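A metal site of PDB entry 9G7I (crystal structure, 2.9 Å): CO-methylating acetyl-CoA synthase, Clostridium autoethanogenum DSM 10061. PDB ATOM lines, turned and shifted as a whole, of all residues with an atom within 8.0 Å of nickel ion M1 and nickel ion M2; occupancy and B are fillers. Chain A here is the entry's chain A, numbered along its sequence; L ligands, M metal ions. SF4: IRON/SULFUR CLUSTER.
The side-chain sulfur (SG) of Cys 488 binds an iron atom (FE4) of the ligand, at 2.4 Å. A ring nitrogen (NE2) of His 495 sits close to a sulfur (S3) of the ligand, at 3.8 Å. The backbone NH (N) of Cys 507 lies close to a sulfur (S1) of the ligand (2.9 Å). The guanidinium group (NH2) of Arg 383 lies close to a sulfur (S2) of the ligand (3.5 Å). The side-chain sulfur (SG) of Cys 507 is bound to an iron atom (FE3) of the ligand (2.5 Å). N of Leu 506 sits close to S1 of the ligand (3.6 Å). SG of Cys 485 is bound to FE1 of the ligand (2.6 Å). The side-chain hydroxyl of Tyr 387 lies close to a sulfur (S2) of the ligand (3.4 Å). The side-chain sulfur (SG) of Cys 497 binds an iron atom (FE2) of the ligand, at 2.8 Å.
Nickel ion M2 is bound by SG of Cys 576 (2.0 Å), SG of Cys 574 (2.1 Å) and SG of Cys 488 (2.4 Å). Slightly farther from nickel ion M2 lies a sulfur (S1) of the ligand (2.9 Å).
Of the 28 residues printed, 3 come within 4 Å of nickel ion M2. The nearest printed residue that does not touch nickel ion M2 is Phe 491 (4.2 Å).
The backbone nitrogen (N) of Cys 576 is bound to nickel ion M1 (1.9 Å). N of Gly 575 binds nickel ion M1 (2.0 Å). SG of Cys 574 is bound to nickel ion M1 (2.3 Å). The side-chain sulfur (SG) of Cys 576 binds nickel ion M1, at 2.7 Å. Nickel ion M1 has four donor atoms within binding distance.
Residues that only touch nickel ion M1: Phe 577 (3.6 Å).
The backbone carbonyl oxygen of Cys 574 lies within hydrogen-bond range of the backbone NH of Gly 616, 3.2 Å away. NE2 of His 495 lies close to SG of Cys 574 (3.7 Å). The guanidinium group (NH2) of Arg 595 sits at hydrogen-bond distance from the backbone carbonyl oxygen (O) of Phe 577, at 3.2 Å. SG of Cys 576 lies close to N of Cys 507 (3.7 Å). O of Cys 576 lies within hydrogen-bond range of NH2 of Arg 595.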
ATOM      1  N   ARG A 383     -10.968  37.592  -6.088  1.00  0.00           N
ATOM      2  CA  ARG A 383     -11.056  36.157  -6.469  1.00  0.00           C
ATOM      3  C   ARG A 383     -12.284  35.958  -7.367  1.00  0.00           C
ATOM      4  O   ARG A 383     -12.143  35.309  -8.414  1.00  0.00           O
ATOM      5  CB  ARG A 383     -11.149  35.275  -5.225  1.00  0.00           C
ATOM      6  CG  ARG A 383     -11.383  33.797  -5.524  1.00  0.00           C
ATOM      7  CD  ARG A 383     -10.213  33.173  -6.266  1.00  0.00           C
ATOM      8  NE  ARG A 383     -10.508  31.818  -6.706  1.00  0.00           N
ATOM      9  CZ  ARG A 383      -9.955  31.249  -7.775  1.00  0.00           C
ATOM     10  NH1 ARG A 383      -9.102  31.927  -8.525  1.00  0.00           N
ATOM     11  NH2 ARG A 383     -10.270  30.001  -8.090  1.00  0.00           N
ATOM     12  N   HIS A 386     -12.183  36.331 -11.279  1.00  0.00           N
ATOM     13  CA  HIS A 386     -11.724  35.172 -12.050  1.00  0.00           C
ATOM     14  C   HIS A 386     -12.914  34.355 -12.545  1.00  0.00           C
ATOM     15  O   HIS A 386     -12.922  33.907 -13.692  1.00  0.00           O
ATOM     16  CB  HIS A 386     -10.770  34.312 -11.192  1.00  0.00           C
ATOM     17  CG  HIS A 386     -10.725  32.858 -11.549  1.00  0.00           C
ATOM     18  ND1 HIS A 386     -10.004  32.407 -12.649  1.00  0.00           N
ATOM     19  CD2 HIS A 386     -11.286  31.794 -10.948  1.00  0.00           C
ATOM     20  CE1 HIS A 386     -10.162  31.095 -12.670  1.00  0.00           C
ATOM     21  NE2 HIS A 386     -10.930  30.675 -11.660  1.00  0.00           N
ATOM     22  N   TYR A 387     -13.916  34.155 -11.681  1.00  0.00           N
ATOM     23  CA  TYR A 387     -15.107  33.381 -12.038  1.00  0.00           C
ATOM     24  C   TYR A 387     -16.002  34.146 -13.013  1.00  0.00           C
ATOM     25  O   TYR A 387     -16.444  33.569 -14.002  1.00  0.00           O
ATOM     26  CB  TYR A 387     -15.883  32.980 -10.769  1.00  0.00           C
ATOM     27  CG  TYR A 387     -15.101  32.041  -9.874  1.00  0.00           C
ATOM     28  CD1 TYR A 387     -14.181  32.536  -8.961  1.00  0.00           C
ATOM     29  CD2 TYR A 387     -15.266  30.666  -9.954  1.00  0.00           C
ATOM     30  CE1 TYR A 387     -13.450  31.685  -8.147  1.00  0.00           C
ATOM     31  CE2 TYR A 387     -14.536  29.801  -9.135  1.00  0.00           C
ATOM     32  CZ  TYR A 387     -13.618  30.318  -8.242  1.00  0.00           C
ATOM     33  OH  TYR A 387     -12.886  29.484  -7.425  1.00  0.00           O
ATOM     34  N   CYS A 485     -12.204  25.137   1.779  1.00  0.00           N
ATOM     35  CA  CYS A 485     -12.907  25.650   0.607  1.00  0.00           C
ATOM     36  C   CYS A 485     -13.245  24.511  -0.350  1.00  0.00           C
ATOM     37  O   CYS A 485     -12.424  23.603  -0.530  1.00  0.00           O
ATOM     38  CB  CYS A 485     -12.081  26.729  -0.089  1.00  0.00           C
ATOM     39  SG  CYS A 485     -12.825  27.333  -1.637  1.00  0.00           S
ATOM     40  N   LEU A 487     -14.885  25.369  -3.560  1.00  0.00           N
ATOM     41  CA  LEU A 487     -15.295  26.066  -4.774  1.00  0.00           C
ATOM     42  C   LEU A 487     -14.747  25.354  -6.013  1.00  0.00           C
ATOM     43  O   LEU A 487     -15.435  25.284  -7.036  1.00  0.00           O
ATOM     44  CB  LEU A 487     -14.825  27.540  -4.723  1.00  0.00           C
ATOM     45  CG  LEU A 487     -15.692  28.599  -5.408  1.00  0.00           C
ATOM     46  CD1 LEU A 487     -17.181  28.455  -5.065  1.00  0.00           C
ATOM     47  CD2 LEU A 487     -15.199  30.007  -5.045  1.00  0.00           C
ATOM     48  N   CYS A 488     -13.572  24.739  -5.895  1.00  0.00           N
ATOM     49  CA  CYS A 488     -12.965  24.007  -7.038  1.00  0.00           C
ATOM     50  C   CYS A 488     -13.655  22.651  -7.238  1.00  0.00           C
ATOM     51  O   CYS A 488     -13.255  21.928  -8.175  1.00  0.00           O
ATOM     52  CB  CYS A 488     -11.489  23.766  -6.790  1.00  0.00           C
ATOM     53  SG  CYS A 488     -10.478  25.254  -7.059  1.00  0.00           S
ATOM     54  N   GLN A 489     -14.642  22.331  -6.403  1.00  0.00           N
ATOM     55  CA  GLN A 489     -15.310  21.035  -6.501  1.00  0.00           C
ATOM     56  C   GLN A 489     -16.195  20.928  -7.766  1.00  0.00           C
ATOM     57  O   GLN A 489     -16.722  19.862  -8.049  1.00  0.00           O
ATOM     58  CB  GLN A 489     -16.142  20.764  -5.232  1.00  0.00           C
ATOM     59  CG  GLN A 489     -16.308  19.277  -4.909  1.00  0.00           C
ATOM     60  CD  GLN A 489     -16.982  19.036  -3.575  1.00  0.00           C
ATOM     61  OE1 GLN A 489     -17.071  19.922  -2.730  1.00  0.00           O
ATOM     62  NE2 GLN A 489     -17.474  17.826  -3.370  1.00  0.00           N
ATOM     63  N   PHE A 491     -15.138  21.120 -10.869  1.00  0.00           N
ATOM     64  CA  PHE A 491     -14.393  20.259 -11.796  1.00  0.00           C
ATOM     65  C   PHE A 491     -13.764  19.072 -11.061  1.00  0.00           C
ATOM     66  O   PHE A 491     -13.811  17.950 -11.575  1.00  0.00           O
ATOM     67  CB  PHE A 491     -13.326  21.061 -12.568  1.00  0.00           C
ATOM     68  CG  PHE A 491     -12.412  21.944 -11.755  1.00  0.00           C
ATOM     69  CD1 PHE A 491     -12.827  23.186 -11.328  1.00  0.00           C
ATOM     70  CD2 PHE A 491     -11.110  21.559 -11.497  1.00  0.00           C
ATOM     71  CE1 PHE A 491     -11.971  24.017 -10.614  1.00  0.00           C
ATOM     72  CE2 PHE A 491     -10.261  22.385 -10.779  1.00  0.00           C
ATOM     73  CZ  PHE A 491     -10.691  23.611 -10.353  1.00  0.00           C
ATOM     74  N   ALA A 492     -13.187  19.298  -9.871  1.00  0.00           N
ATOM     75  CA  ALA A 492     -12.582  18.232  -9.071  1.00  0.00           C
ATOM     76  C   ALA A 492     -13.571  17.762  -7.994  1.00  0.00           C
ATOM     77  O   ALA A 492     -13.587  18.343  -6.910  1.00  0.00           O
ATOM     78  CB  ALA A 492     -11.317  18.733  -8.401  1.00  0.00           C
ATOM     79  N   HIS A 495     -12.050  17.403  -4.319  1.00  0.00           N
ATOM     80  CA  HIS A 495     -11.075  18.388  -3.841  1.00  0.00           C
ATOM     81  C   HIS A 495     -11.625  19.208  -2.693  1.00  0.00           C
ATOM     82  O   HIS A 495     -12.665  19.867  -2.836  1.00  0.00           O
ATOM     83  CB  HIS A 495     -10.642  19.319  -4.979  1.00  0.00           C
ATOM     84  CG  HIS A 495      -9.650  20.354  -4.548  1.00  0.00           C
ATOM     85  ND1 HIS A 495      -8.306  20.063  -4.450  1.00  0.00           N
ATOM     86  CD2 HIS A 495      -9.848  21.643  -4.176  1.00  0.00           C
ATOM     87  CE1 HIS A 495      -7.724  21.181  -4.047  1.00  0.00           C
ATOM     88  NE2 HIS A 495      -8.611  22.154  -3.859  1.00  0.00           N
ATOM     89  N   CYS A 497      -9.950  21.997  -0.346  1.00  0.00           N
ATOM     90  CA  CYS A 497      -8.701  22.764  -0.097  1.00  0.00           C
ATOM     91  C   CYS A 497      -8.636  23.315   1.326  1.00  0.00           C
ATOM     92  O   CYS A 497      -9.389  24.258   1.621  1.00  0.00           O
ATOM     93  CB  CYS A 497      -8.558  23.922  -1.094  1.00  0.00           C
ATOM     94  SG  CYS A 497      -6.877  24.575  -1.243  1.00  0.00           S
ATOM     95  N   GLY A 505      -4.390  28.648  -0.299  1.00  0.00           N
ATOM     96  CA  GLY A 505      -5.257  28.000  -1.301  1.00  0.00           C
ATOM     97  C   GLY A 505      -4.482  27.738  -2.572  1.00  0.00           C
ATOM     98  O   GLY A 505      -3.830  28.687  -3.064  1.00  0.00           O
ATOM     99  N   LEU A 506      -4.528  26.519  -3.078  1.00  0.00           N
ATOM    100  CA  LEU A 506      -3.744  26.156  -4.262  1.00  0.00           C
ATOM    101  C   LEU A 506      -3.913  27.188  -5.384  1.00  0.00           C
ATOM    102  O   LEU A 506      -3.036  27.322  -6.237  1.00  0.00           O
ATOM    103  CB  LEU A 506      -4.099  24.752  -4.779  1.00  0.00           C
ATOM    104  CG  LEU A 506      -4.149  23.607  -3.752  1.00  0.00           C
ATOM    105  CD1 LEU A 506      -4.286  22.269  -4.443  1.00  0.00           C
ATOM    106  CD2 LEU A 506      -2.921  23.592  -2.850  1.00  0.00           C
ATOM    107  N   CYS A 507      -5.010  27.933  -5.397  1.00  0.00           N
ATOM    108  CA  CYS A 507      -5.161  28.879  -6.540  1.00  0.00           C
ATOM    109  C   CYS A 507      -4.227  30.073  -6.365  1.00  0.00           C
ATOM    110  O   CYS A 507      -3.919  30.732  -7.381  1.00  0.00           O
ATOM    111  CB  CYS A 507      -6.592  29.364  -6.670  1.00  0.00           C
ATOM    112  SG  CYS A 507      -7.122  30.298  -5.220  1.00  0.00           S
ATOM    113  N   GLY A 508      -3.750  30.319  -5.141  1.00  0.00           N
ATOM    114  CA  GLY A 508      -2.786  31.403  -4.881  1.00  0.00           C
ATOM    115  C   GLY A 508      -3.478  32.677  -4.409  1.00  0.00           C
ATOM    116  O   GLY A 508      -2.777  33.587  -3.940  1.00  0.00           O
ATOM    117  N   THR A 572      -5.113  16.807  -1.751  1.00  0.00           N
ATOM    118  CA  THR A 572      -5.533  16.721  -3.157  1.00  0.00           C
ATOM    119  C   THR A 572      -5.304  18.037  -3.896  1.00  0.00           C
ATOM    120  O   THR A 572      -5.293  19.102  -3.283  1.00  0.00           O
ATOM    121  CB  THR A 572      -7.005  16.270  -3.240  1.00  0.00           C
ATOM    122  OG1 THR A 572      -7.793  17.089  -2.374  1.00  0.00           O
ATOM    123  CG2 THR A 572      -7.199  14.804  -2.886  1.00  0.00           C
ATOM    124  N   SER A 573      -5.094  17.957  -5.215  1.00  0.00           N
ATOM    125  CA  SER A 573      -4.858  19.128  -6.060  1.00  0.00           C
ATOM    126  C   SER A 573      -6.050  19.324  -7.025  1.00  0.00           C
ATOM    127  O   SER A 573      -6.725  18.355  -7.363  1.00  0.00           O
ATOM    128  CB  SER A 573      -3.546  18.986  -6.830  1.00  0.00           C
ATOM    129  OG  SER A 573      -2.463  18.764  -5.941  1.00  0.00           O
ATOM    130  N   CYS A 574      -6.316  20.569  -7.452  1.00  0.00           N
ATOM    131  CA  CYS A 574      -7.447  20.876  -8.323  1.00  0.00           C
ATOM    132  C   CYS A 574      -7.057  21.129  -9.802  1.00  0.00           C
ATOM    133  O   CYS A 574      -7.152  20.208 -10.615  1.00  0.00           O
ATOM    134  CB  CYS A 574      -8.251  22.046  -7.750  1.00  0.00           C
ATOM    135  SG  CYS A 574      -7.238  23.385  -7.077  1.00  0.00           S
ATOM    136  N   GLY A 575      -6.626  22.349 -10.143  1.00  0.00           N
ATOM    137  CA  GLY A 575      -6.246  22.674 -11.507  1.00  0.00           C
ATOM    138  C   GLY A 575      -5.851  24.125 -11.740  1.00  0.00           C
ATOM    139  O   GLY A 575      -5.511  24.507 -12.865  1.00  0.00           O
ATOM    140  N   CYS A 576      -5.900  24.954 -10.690  1.00  0.00           N
ATOM    141  CA  CYS A 576      -5.554  26.380 -10.747  1.00  0.00           C
ATOM    142  C   CYS A 576      -4.165  26.679 -10.193  1.00  0.00           C
ATOM    143  O   CYS A 576      -3.820  27.849 -10.039  1.00  0.00           O
ATOM    144  CB  CYS A 576      -6.617  27.182 -10.004  1.00  0.00           C
ATOM    145  SG  CYS A 576      -6.928  26.595  -8.320  1.00  0.00           S
ATOM    146  N   PHE A 577      -3.378  25.629  -9.949  1.00  0.00           N
ATOM    147  CA  PHE A 577      -2.012  25.792  -9.387  1.00  0.00           C
ATOM    148  C   PHE A 577      -1.121  26.524 -10.390  1.00  0.00           C
ATOM    149  O   PHE A 577      -1.095  26.132 -11.569  1.00  0.00           O
ATOM    150  CB  PHE A 577      -1.422  24.432  -9.000  1.00  0.00           C
ATOM    151  CG  PHE A 577      -1.801  23.234  -9.845  1.00  0.00           C
ATOM    152  CD1 PHE A 577      -1.272  23.056 -11.111  1.00  0.00           C
ATOM    153  CD2 PHE A 577      -2.650  22.258  -9.355  1.00  0.00           C
ATOM    154  CE1 PHE A 577      -1.601  21.954 -11.875  1.00  0.00           C
ATOM    155  CE2 PHE A 577      -2.986  21.150 -10.115  1.00  0.00           C
ATOM    156  CZ  PHE A 577      -2.455  20.989 -11.378  1.00  0.00           C
ATOM    157  N   GLU A 578      -0.408  27.555  -9.943  1.00  0.00           N
ATOM    158  CA  GLU A 578       0.524  28.260 -10.866  1.00  0.00           C
ATOM    159  C   GLU A 578       1.851  27.500 -10.928  1.00  0.00           C
ATOM    160  O   GLU A 578       2.475  27.488 -12.009  1.00  0.00           O
ATOM    161  CB  GLU A 578       0.691  29.707 -10.406  1.00  0.00           C
ATOM    162  CG  GLU A 578       1.917  30.363 -11.004  1.00  0.00           C
ATOM    163  CD  GLU A 578       1.864  30.686 -12.487  1.00  0.00           C
ATOM    164  OE1 GLU A 578       1.013  31.495 -12.879  1.00  0.00           O
ATOM    165  OE2 GLU A 578       2.706  30.147 -13.241  1.00  0.00           O
ATOM    166  N   ARG A 595       3.532  27.820 -14.606  1.00  0.00           N
ATOM    167  CA  ARG A 595       2.659  27.733 -15.772  1.00  0.00           C
ATOM    168  C   ARG A 595       3.225  28.446 -17.009  1.00  0.00           C
ATOM    169  O   ARG A 595       2.895  28.081 -18.136  1.00  0.00           O
ATOM    170  CB  ARG A 595       1.268  28.303 -15.436  1.00  0.00           C
ATOM    171  CG  ARG A 595       0.151  27.808 -16.363  1.00  0.00           C
ATOM    172  CD  ARG A 595      -1.145  28.602 -16.222  1.00  0.00           C
ATOM    173  NE  ARG A 595      -1.812  28.375 -14.929  1.00  0.00           N
ATOM    174  CZ  ARG A 595      -1.708  29.160 -13.859  1.00  0.00           C
ATOM    175  NH1 ARG A 595      -0.941  30.253 -13.894  1.00  0.00           N
ATOM    176  NH2 ARG A 595      -2.362  28.861 -12.748  1.00  0.00           N
ATOM    177  N   THR A 614      -1.114  15.912 -11.096  1.00  0.00           N
ATOM    178  CA  THR A 614      -1.371  16.457  -9.735  1.00  0.00           C
ATOM    179  C   THR A 614      -2.849  16.713  -9.445  1.00  0.00           C
ATOM    180  O   THR A 614      -3.323  16.253  -8.392  1.00  0.00           O
ATOM    181  CB  THR A 614      -0.563  17.753  -9.622  1.00  0.00           C
ATOM    182  OG1 THR A 614      -1.043  18.657 -10.622  1.00  0.00           O
ATOM    183  CG2 THR A 614       0.919  17.529  -9.783  1.00  0.00           C
ATOM    184  N   GLY A 615      -3.541  17.412 -10.345  1.00  0.00           N
ATOM    185  CA  GLY A 615      -4.948  17.788 -10.100  1.00  0.00           C
ATOM    186  C   GLY A 615      -5.948  16.662 -10.190  1.00  0.00           C
ATOM    187  O   GLY A 615      -5.543  15.491 -10.058  1.00  0.00           O
ATOM    188  N   GLY A 616      -7.212  17.006 -10.417  1.00  0.00           N
ATOM    189  CA  GLY A 616      -8.320  16.060 -10.495  1.00  0.00           C
ATOM    190  C   GLY A 616      -8.922  15.647  -9.169  1.00  0.00           C
ATOM    191  O   GLY A 616      -9.774  14.757  -9.126  1.00  0.00           O
ATOM    192  N   GLY A 625       0.418  20.568  -6.341  1.00  0.00           N
ATOM    193  CA  GLY A 625       0.185  21.884  -6.928  1.00  0.00           C
ATOM    194  C   GLY A 625       0.128  22.952  -5.857  1.00  0.00           C
ATOM    195  O   GLY A 625      -0.460  22.723  -4.802  1.00  0.00           O
ATOM    196  N   HIS A 626       0.746  24.109  -6.099  1.00  0.00           N
ATOM    197  CA  HIS A 626       0.783  25.196  -5.113  1.00  0.00           C
ATOM    198  C   HIS A 626       1.004  26.560  -5.794  1.00  0.00           C
ATOM    199  O   HIS A 626       1.358  26.630  -6.964  1.00  0.00           O
ATOM    200  CB  HIS A 626       1.906  24.927  -4.101  1.00  0.00           C
ATOM    201  CG  HIS A 626       3.245  24.726  -4.741  1.00  0.00           C
ATOM    202  ND1 HIS A 626       4.147  25.767  -4.848  1.00  0.00           N
ATOM    203  CD2 HIS A 626       3.780  23.631  -5.312  1.00  0.00           C
ATOM    204  CE1 HIS A 626       5.202  25.269  -5.476  1.00  0.00           C
ATOM    205  NE2 HIS A 626       5.025  23.978  -5.769  1.00  0.00           N
HETATM  206 FE1  SF4 L   1     -10.611  27.607  -2.877  1.00  0.00          FE
HETATM  207 FE2  SF4 L   1      -8.396  26.229  -2.892  1.00  0.00          FE
HETATM  208 FE3  SF4 L   1      -8.500  28.561  -4.145  1.00  0.00          FE
HETATM  209 FE4  SF4 L   1      -9.823  26.463  -5.089  1.00  0.00          FE
HETATM  210  S1  SF4 L   1      -7.535  26.650  -4.976  1.00  0.00           S
HETATM  211  S2  SF4 L   1     -10.655  28.596  -4.960  1.00  0.00           S
HETATM  212  S3  SF4 L   1     -10.494  25.341  -3.208  1.00  0.00           S
HETATM  213  S4  SF4 L   1      -8.642  28.271  -1.881  1.00  0.00           S
HETATM  214 NI    NI M   1      -6.497  24.053  -9.120  1.00  0.00          NI
HETATM  215 NI    NI M   2      -8.136  25.203  -7.430  1.00  0.00          NI
